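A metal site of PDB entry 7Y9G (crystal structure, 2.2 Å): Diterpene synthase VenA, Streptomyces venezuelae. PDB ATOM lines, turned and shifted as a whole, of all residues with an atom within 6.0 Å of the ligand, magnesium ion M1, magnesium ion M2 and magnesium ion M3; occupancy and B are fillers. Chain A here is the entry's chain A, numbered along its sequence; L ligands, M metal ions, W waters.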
ATOM      1  N   THR A 103       3.648   2.865  -7.009  1.00  0.00           N
ATOM      2  CA  THR A 103       3.159   2.184  -5.807  1.00  0.00           C
ATOM      3  C   THR A 103       2.284   1.012  -6.250  1.00  0.00           C
ATOM      4  O   THR A 103       2.379  -0.049  -5.622  1.00  0.00           O
ATOM      5  CB  THR A 103       2.434   3.136  -4.852  1.00  0.00           C
ATOM      6  OG1 THR A 103       3.335   4.181  -4.478  1.00  0.00           O
ATOM      7  CG2 THR A 103       1.986   2.425  -3.602  1.00  0.00           C
ATOM      8  N   ASP A 106       4.896  -1.422  -7.295  1.00  0.00           N
ATOM      9  CA  ASP A 106       5.577  -1.933  -6.080  1.00  0.00           C
ATOM     10  C   ASP A 106       4.723  -3.004  -5.423  1.00  0.00           C
ATOM     11  O   ASP A 106       5.303  -3.999  -4.980  1.00  0.00           O
ATOM     12  CB  ASP A 106       5.831  -0.864  -5.027  1.00  0.00           C
ATOM     13  CG  ASP A 106       6.717  -1.397  -3.907  1.00  0.00           C
ATOM     14  OD1 ASP A 106       7.899  -1.623  -4.192  1.00  0.00           O
ATOM     15  OD2 ASP A 106       6.199  -1.630  -2.769  1.00  0.00           O
ATOM     16  N   SER A 107       3.403  -2.766  -5.331  1.00  0.00           N
ATOM     17  CA  SER A 107       2.433  -3.672  -4.667  1.00  0.00           C
ATOM     18  C   SER A 107       2.233  -4.945  -5.504  1.00  0.00           C
ATOM     19  O   SER A 107       2.134  -5.997  -4.893  1.00  0.00           O
ATOM     20  CB  SER A 107       1.108  -2.989  -4.400  1.00  0.00           C
ATOM     21  OG  SER A 107       1.287  -1.936  -3.468  1.00  0.00           O
ATOM     22  N   SER A 110       5.742  -7.166  -5.460  1.00  0.00           N
ATOM     23  CA  SER A 110       6.041  -7.631  -4.078  1.00  0.00           C
ATOM     24  C   SER A 110       4.967  -8.622  -3.631  1.00  0.00           C
ATOM     25  O   SER A 110       5.090  -9.159  -2.512  1.00  0.00           O
ATOM     26  CB  SER A 110       6.153  -6.465  -3.124  1.00  0.00           C
ATOM     27  OG  SER A 110       4.981  -6.328  -2.327  1.00  0.00           O
ATOM     28  N   PHE A 176      15.148   0.936 -10.794  1.00  0.00           N
ATOM     29  CA  PHE A 176      13.971   0.512  -9.982  1.00  0.00           C
ATOM     30  C   PHE A 176      13.702  -0.969 -10.257  1.00  0.00           C
ATOM     31  O   PHE A 176      13.591  -1.759  -9.283  1.00  0.00           O
ATOM     32  CB  PHE A 176      12.764   1.407 -10.275  1.00  0.00           C
ATOM     33  CG  PHE A 176      11.494   0.981  -9.568  1.00  0.00           C
ATOM     34  CD1 PHE A 176      11.375   1.087  -8.185  1.00  0.00           C
ATOM     35  CD2 PHE A 176      10.434   0.437 -10.291  1.00  0.00           C
ATOM     36  CE1 PHE A 176      10.221   0.650  -7.547  1.00  0.00           C
ATOM     37  CE2 PHE A 176       9.278   0.022  -9.649  1.00  0.00           C
ATOM     38  CZ  PHE A 176       9.185   0.119  -8.278  1.00  0.00           C
ATOM     39  N   CYS A 180      13.676  -4.170  -7.817  1.00  0.00           N
ATOM     40  CA  CYS A 180      12.505  -5.073  -7.596  1.00  0.00           C
ATOM     41  C   CYS A 180      12.879  -6.526  -7.891  1.00  0.00           C
ATOM     42  O   CYS A 180      12.462  -7.432  -7.140  1.00  0.00           O
ATOM     43  CB  CYS A 180      11.314  -4.650  -8.460  1.00  0.00           C
ATOM     44  SG  CYS A 180      10.654  -3.020  -8.002  1.00  0.00           S
ATOM     45  N   GLU A 183      14.942  -8.095  -5.087  1.00  0.00           N
ATOM     46  CA  GLU A 183      14.016  -8.355  -3.946  1.00  0.00           C
ATOM     47  C   GLU A 183      13.218  -9.622  -4.232  1.00  0.00           C
ATOM     48  O   GLU A 183      13.081 -10.479  -3.341  1.00  0.00           O
ATOM     49  CB  GLU A 183      13.040  -7.204  -3.752  1.00  0.00           C
ATOM     50  CG  GLU A 183      13.679  -5.898  -3.335  1.00  0.00           C
ATOM     51  CD  GLU A 183      12.713  -4.723  -3.200  1.00  0.00           C
ATOM     52  OE1 GLU A 183      13.010  -3.812  -2.406  1.00  0.00           O
ATOM     53  OE2 GLU A 183      11.643  -4.711  -3.889  1.00  0.00           O
ATOM     54  N   ARG A 202      18.332  -1.407  -2.061  1.00  0.00           N
ATOM     55  CA  ARG A 202      17.181  -0.487  -1.853  1.00  0.00           C
ATOM     56  C   ARG A 202      17.442   0.868  -2.506  1.00  0.00           C
ATOM     57  O   ARG A 202      16.455   1.579  -2.744  1.00  0.00           O
ATOM     58  CB  ARG A 202      16.868  -0.396  -0.356  1.00  0.00           C
ATOM     59  CG  ARG A 202      16.263  -1.659   0.209  1.00  0.00           C
ATOM     60  CD  ARG A 202      14.771  -1.619   0.004  1.00  0.00           C
ATOM     61  NE  ARG A 202      14.106  -0.857   1.043  1.00  0.00           N
ATOM     62  CZ  ARG A 202      12.995  -0.138   0.891  1.00  0.00           C
ATOM     63  NH1 ARG A 202      12.413  -0.026  -0.293  1.00  0.00           N
ATOM     64  NH2 ARG A 202      12.476   0.488   1.932  1.00  0.00           N
ATOM     65  N   SER A 205      15.766  -0.149  -5.602  1.00  0.00           N
ATOM     66  CA  SER A 205      14.378  -0.641  -5.469  1.00  0.00           C
ATOM     67  C   SER A 205      13.478   0.470  -4.892  1.00  0.00           C
ATOM     68  O   SER A 205      12.269   0.462  -5.189  1.00  0.00           O
ATOM     69  CB  SER A 205      14.319  -1.934  -4.713  1.00  0.00           C
ATOM     70  OG  SER A 205      14.440  -1.764  -3.310  1.00  0.00           O
ATOM     71  N   PHE A 206      14.046   1.379  -4.109  1.00  0.00           N
ATOM     72  CA  PHE A 206      13.345   2.532  -3.491  1.00  0.00           C
ATOM     73  C   PHE A 206      13.137   3.622  -4.535  1.00  0.00           C
ATOM     74  O   PHE A 206      12.389   4.539  -4.271  1.00  0.00           O
ATOM     75  CB  PHE A 206      14.106   3.081  -2.270  1.00  0.00           C
ATOM     76  CG  PHE A 206      13.322   4.026  -1.404  1.00  0.00           C
ATOM     77  CD1 PHE A 206      12.358   3.553  -0.528  1.00  0.00           C
ATOM     78  CD2 PHE A 206      13.544   5.398  -1.459  1.00  0.00           C
ATOM     79  CE1 PHE A 206      11.625   4.429   0.259  1.00  0.00           C
ATOM     80  CE2 PHE A 206      12.823   6.269  -0.666  1.00  0.00           C
ATOM     81  CZ  PHE A 206      11.853   5.790   0.183  1.00  0.00           C
ATOM     82  N   ASN A 247      11.072   4.533   6.133  1.00  0.00           N
ATOM     83  CA  ASN A 247      10.086   3.690   5.447  1.00  0.00           C
ATOM     84  C   ASN A 247      10.132   2.296   6.088  1.00  0.00           C
ATOM     85  O   ASN A 247       9.076   1.753   6.312  1.00  0.00           O
ATOM     86  CB  ASN A 247      10.261   3.660   3.924  1.00  0.00           C
ATOM     87  CG  ASN A 247       9.252   2.738   3.268  1.00  0.00           C
ATOM     88  OD1 ASN A 247       9.452   1.532   3.228  1.00  0.00           O
ATOM     89  ND2 ASN A 247       8.137   3.295   2.832  1.00  0.00           N
ATOM     90  N   ASP A 248      11.300   1.720   6.353  1.00  0.00           N
ATOM     91  CA  ASP A 248      11.372   0.347   6.933  1.00  0.00           C
ATOM     92  C   ASP A 248      10.634   0.319   8.271  1.00  0.00           C
ATOM     93  O   ASP A 248       9.886  -0.650   8.512  1.00  0.00           O
ATOM     94  CB  ASP A 248      12.811  -0.140   7.057  1.00  0.00           C
ATOM     95  CG  ASP A 248      13.444  -0.453   5.725  1.00  0.00           C
ATOM     96  OD1 ASP A 248      12.746  -0.346   4.708  1.00  0.00           O
ATOM     97  OD2 ASP A 248      14.673  -0.723   5.705  1.00  0.00           O
ATOM     98  N   SER A 251       6.745   1.005   7.612  1.00  0.00           N
ATOM     99  CA  SER A 251       6.181  -0.047   6.724  1.00  0.00           C
ATOM    100  C   SER A 251       6.369  -1.447   7.334  1.00  0.00           C
ATOM    101  O   SER A 251       5.850  -2.393   6.740  1.00  0.00           O
ATOM    102  CB  SER A 251       6.707   0.075   5.296  1.00  0.00           C
ATOM    103  OG  SER A 251       8.067  -0.306   5.151  1.00  0.00           O
ATOM    104  N   TRP A 252       7.003  -1.598   8.515  1.00  0.00           N
ATOM    105  CA  TRP A 252       7.269  -2.960   9.069  1.00  0.00           C
ATOM    106  C   TRP A 252       5.960  -3.716   9.351  1.00  0.00           C
ATOM    107  O   TRP A 252       5.900  -4.914   9.043  1.00  0.00           O
ATOM    108  CB  TRP A 252       8.170  -2.903  10.323  1.00  0.00           C
ATOM    109  CG  TRP A 252       8.359  -4.242  10.980  1.00  0.00           C
ATOM    110  CD1 TRP A 252       8.021  -4.570  12.259  1.00  0.00           C
ATOM    111  CD2 TRP A 252       8.886  -5.452  10.399  1.00  0.00           C
ATOM    112  NE1 TRP A 252       8.344  -5.879  12.522  1.00  0.00           N
ATOM    113  CE2 TRP A 252       8.848  -6.452  11.393  1.00  0.00           C
ATOM    114  CE3 TRP A 252       9.398  -5.791   9.137  1.00  0.00           C
ATOM    115  CZ2 TRP A 252       9.328  -7.749  11.181  1.00  0.00           C
ATOM    116  CZ3 TRP A 252       9.854  -7.080   8.914  1.00  0.00           C
ATOM    117  CH2 TRP A 252       9.812  -8.046   9.924  1.00  0.00           C
ATOM    118  N   LYS A 254       3.315  -3.885   7.827  1.00  0.00           N
ATOM    119  CA  LYS A 254       2.742  -4.469   6.592  1.00  0.00           C
ATOM    120  C   LYS A 254       3.745  -5.458   5.988  1.00  0.00           C
ATOM    121  O   LYS A 254       3.311  -6.468   5.447  1.00  0.00           O
ATOM    122  CB  LYS A 254       2.295  -3.366   5.622  1.00  0.00           C
ATOM    123  CG  LYS A 254       3.208  -3.035   4.454  1.00  0.00           C
ATOM    124  CD  LYS A 254       2.465  -2.770   3.149  1.00  0.00           C
ATOM    125  CE  LYS A 254       3.317  -2.135   2.066  1.00  0.00           C
ATOM    126  NZ  LYS A 254       4.264  -3.096   1.462  1.00  0.00           N
ATOM    127  N   GLU A 255       5.053  -5.208   6.086  1.00  0.00           N
ATOM    128  CA  GLU A 255       6.073  -6.086   5.456  1.00  0.00           C
ATOM    129  C   GLU A 255       6.195  -7.378   6.281  1.00  0.00           C
ATOM    130  O   GLU A 255       6.440  -8.435   5.689  1.00  0.00           O
ATOM    131  CB  GLU A 255       7.358  -5.280   5.251  1.00  0.00           C
ATOM    132  CG  GLU A 255       7.173  -4.249   4.162  1.00  0.00           C
ATOM    133  CD  GLU A 255       8.325  -3.285   3.977  1.00  0.00           C
ATOM    134  OE1 GLU A 255       9.318  -3.440   4.691  1.00  0.00           O
ATOM    135  OE2 GLU A 255       8.201  -2.372   3.135  1.00  0.00           O
ATOM    136  N   GLN A 258       3.382  -9.441   5.034  1.00  0.00           N
ATOM    137  CA  GLN A 258       3.602  -9.794   3.598  1.00  0.00           C
ATOM    138  C   GLN A 258       4.896 -10.592   3.384  1.00  0.00           C
ATOM    139  O   GLN A 258       5.178 -10.945   2.229  1.00  0.00           O
ATOM    140  CB  GLN A 258       3.592  -8.510   2.771  1.00  0.00           C
ATOM    141  CG  GLN A 258       2.220  -7.859   2.678  1.00  0.00           C
ATOM    142  CD  GLN A 258       2.228  -6.548   1.923  1.00  0.00           C
ATOM    143  OE1 GLN A 258       3.228  -6.158   1.322  1.00  0.00           O
ATOM    144  NE2 GLN A 258       1.125  -5.829   1.991  1.00  0.00           N
ATOM    145  N   ASP A 260       8.022  -9.851   3.271  1.00  0.00           N
ATOM    146  CA  ASP A 260       9.090  -9.128   2.519  1.00  0.00           C
ATOM    147  C   ASP A 260      10.412  -9.236   3.295  1.00  0.00           C
ATOM    148  O   ASP A 260      10.403  -9.173   4.543  1.00  0.00           O
ATOM    149  CB  ASP A 260       8.740  -7.660   2.295  1.00  0.00           C
ATOM    150  CG  ASP A 260       7.607  -7.467   1.302  1.00  0.00           C
ATOM    151  OD1 ASP A 260       7.437  -8.352   0.407  1.00  0.00           O
ATOM    152  OD2 ASP A 260       6.893  -6.464   1.429  1.00  0.00           O
ATOM    153  N   MET A 262      13.410  -7.476   2.142  1.00  0.00           N
ATOM    154  CA  MET A 262      14.285  -6.306   1.845  1.00  0.00           C
ATOM    155  C   MET A 262      13.894  -5.121   2.741  1.00  0.00           C
ATOM    156  O   MET A 262      13.532  -4.025   2.234  1.00  0.00           O
ATOM    157  CB  MET A 262      14.224  -5.972   0.353  1.00  0.00           C
ATOM    158  CG  MET A 262      15.463  -5.271  -0.145  1.00  0.00           C
ATOM    159  SD  MET A 262      16.982  -6.276  -0.057  1.00  0.00           S
ATOM    160  CE  MET A 262      16.574  -7.678  -1.093  1.00  0.00           C
ATOM    161  N   ARG A 335      -1.866   2.408   3.976  1.00  0.00           N
ATOM    162  CA  ARG A 335      -0.941   1.392   3.419  1.00  0.00           C
ATOM    163  C   ARG A 335      -0.167   0.733   4.584  1.00  0.00           C
ATOM    164  O   ARG A 335       0.145  -0.440   4.481  1.00  0.00           O
ATOM    165  CB  ARG A 335      -0.006   2.056   2.406  1.00  0.00           C
ATOM    166  CG  ARG A 335       0.907   1.120   1.642  1.00  0.00           C
ATOM    167  CD  ARG A 335       1.766   1.868   0.629  1.00  0.00           C
ATOM    168  NE  ARG A 335       2.678   0.980  -0.092  1.00  0.00           N
ATOM    169  CZ  ARG A 335       2.305   0.085  -1.013  1.00  0.00           C
ATOM    170  NH1 ARG A 335       3.222  -0.663  -1.602  1.00  0.00           N
ATOM    171  NH2 ARG A 335       1.026  -0.044  -1.357  1.00  0.00           N
ATOM    172  N   TYR A 336       0.140   1.468   5.656  1.00  0.00           N
ATOM    173  CA  TYR A 336       0.988   0.994   6.780  1.00  0.00           C
ATOM    174  C   TYR A 336       0.131   0.734   8.024  1.00  0.00           C
ATOM    175  O   TYR A 336       0.392  -0.239   8.766  1.00  0.00           O
ATOM    176  CB  TYR A 336       2.125   1.986   7.037  1.00  0.00           C
ATOM    177  CG  TYR A 336       2.980   2.270   5.819  1.00  0.00           C
ATOM    178  CD1 TYR A 336       3.185   1.319   4.829  1.00  0.00           C
ATOM    179  CD2 TYR A 336       3.568   3.499   5.650  1.00  0.00           C
ATOM    180  CE1 TYR A 336       3.969   1.595   3.710  1.00  0.00           C
ATOM    181  CE2 TYR A 336       4.338   3.791   4.538  1.00  0.00           C
ATOM    182  CZ  TYR A 336       4.539   2.838   3.557  1.00  0.00           C
ATOM    183  OH  TYR A 336       5.296   3.171   2.469  1.00  0.00           O
HETATM  184  P1  LIG L   1       8.935  -0.017  -0.248  1.00  0.00           P
HETATM  185  O1  LIG L   1       9.951   0.988  -0.699  1.00  0.00           O
HETATM  186  O2  LIG L   1       9.209  -0.612   1.108  1.00  0.00           O
HETATM  187  O3  LIG L   1       8.593  -1.141  -1.254  1.00  0.00           O
HETATM  188  O4  LIG L   1       7.557   0.887   0.001  1.00  0.00           O
HETATM  189  P2  LIG L   1       6.293   0.340   0.857  1.00  0.00           P
HETATM  190  O5  LIG L   1       6.842   0.321   2.282  1.00  0.00           O
HETATM  191  O6  LIG L   1       5.204   1.345   0.715  1.00  0.00           O
HETATM  192  O7  LIG L   1       5.996  -1.033   0.271  1.00  0.00           O
HETATM  193 MG    MG M   1       8.652  -0.364   3.080  1.00  0.00          MG
HETATM  194 MG    MG M   2       6.964  -2.403  -0.993  1.00  0.00          MG
HETATM  195 MG    MG M   3       9.501  -1.927  -2.936  1.00  0.00          MG
HETATM  196  O   HOH W   1       7.488  -3.593   0.636  1.00  0.00           O
HETATM  197  O   HOH W   2      10.280   0.111  -3.399  1.00  0.00           O
HETATM  198  O   HOH W   3      11.265  -2.941   1.110  1.00  0.00           O
HETATM  199  O   HOH W   4       5.388  -3.795  -1.266  1.00  0.00           O
HETATM  200  O   HOH W   5      11.065  -2.521  -1.745  1.00  0.00           O
HETATM  201  O   HOH W   6       8.705   3.740  -1.175  1.00  0.00           O
HETATM  202  O   HOH W   7       8.260  -3.448  -2.267  1.00  0.00           O
HETATM  203  O   HOH W   8      10.407  -2.707  -4.516  1.00  0.00           O
HETATM  204  O   HOH W   9      10.368  -1.276   3.822  1.00  0.00           O
HETATM  205  O   HOH W  10       5.550   2.739  -2.379  1.00  0.00           O
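Merely in contact with magnesium ion M3: Glu 183 (3.6 Å). The nearest printed residue that does not touch magnesium ion M3 is Ser 205 (4.3 Å).
Lys 254 touches magnesium ion M2. Of the 21 residues printed, 2 come within 4 Å of magnesium ion M2. The nearest printed residue that does not touch magnesium ion M2 is Arg 335 (4.2 Å).
Of the 21 residues printed, 3 come within 4 Å of magnesium ion M1. The nearest printed residue that does not touch magnesium ion M1 is Arg 202 (4.1 Å).
An oxygen (O6) of the ligand is in hydrogen-bond range of the side-chain hydroxyl (OH) of Tyr 336 (2.5 Å). The guanidinium group (NE) of Arg 335 is in salt-bridge range of an oxygen (O6) of the ligand (2.7 Å). NH1 of Arg 202 is in salt-bridge range of O1 of the ligand, 2.7 Å away. An oxygen (O7) of the ligand sits close to the side-chain amino group (NZ) of Lys 254 (2.9 Å).
The side-chain carboxylate (OD2) of Asp 106 lies close to the guanidinium group (NH1) of Arg 335, 3.3 Å away. The backbone NH (N) of Asp 260 sits at hydrogen-bond distance from the backbone carbonyl oxygen (O) of Glu 255 (3.2 Å). OH of Tyr 336 lies within hydrogen-bond range of ND2 of Asn 247, at 2.9 Å. NH2 of Arg 202 lies close to OD1 of Asn 247. The side-chain hydroxyl (OG) of Ser 107 lies within hydrogen-bond range of the guanidinium group (NH2) of Arg 335. The side-chain carboxylate (OD1) of Asp 248 is in salt-bridge range of the guanidinium group (NH2) of Arg 202 (2.9 Å). The backbone carbonyl oxygen (O) of Met 262 sits at hydrogen-bond distance from the guanidinium group (NE) of Arg 202 (3.4 Å). OE1 of Glu 183 sits at hydrogen-bond distance from OG of Ser 205, at 2.7 Å.
Water W9 lies within hydrogen-bond range of the side-chain carboxylate of Glu 255, the side-chain carboxylate of Asp 248 and the guanidinium group of Arg 202. Water W4 lies within hydrogen-bond range of the side-chain hydroxyl of Ser 110 (2.8 Å) and the side-chain amino group of Lys 254 (3.0 Å). Water W5 lies within hydrogen-bond range of OE1 of Glu 183 (2.4 Å) and NH1 of Arg 202 (3.2 Å). Water W8 bridges the side-chain carboxylate of Glu 183 (2.4 Å) and the side-chain sulfur of Cys 180 (3.5 Å). Water W3 lies within hydrogen-bond range of the backbone carbonyl oxygen (O) of Met 262 (2.8 Å) and the guanidinium group (NH1) of Arg 202 (3.4 Å). Water W10 bridges the side-chain hydroxyl of Thr 103 and an oxygen (O6) of the ligand.
Magnesium ion M1 is bound by OE2 of Glu 255, OD1 of Asn 247, O2 of the ligand, water W9, O5 of the ligand and OG of Ser 251.
Magnesium ion M3 is bound by water W8, water W5, the side-chain carboxylate (OD1) of Asp 106, an oxygen (O3) of the ligand, water W7 and water W2.
Merely in contact with the ligand: Phe 206 (3.5 Å). Hydrophobic or aromatic side chains that line the ligand: Phe 206 and Tyr 336. Nine residues have an atom within 4 Å of the ligand: Asp 106, Arg 202, Phe 206, Asn 247, Ser 251, Lys 254, Glu 255, Arg 335 and Tyr 336. The nearest printed residue that does not touch the ligand is Asp 248 (5.1 Å).
Magnesium ion M2 is bound by O3 of the ligand (2.1 Å), OD2 of Asp 106 (2.1 Å), water W1 (2.1 Å), water W7 (2.1 Å), O7 of the ligand (2.1 Å) and water W4 (2.1 Å).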
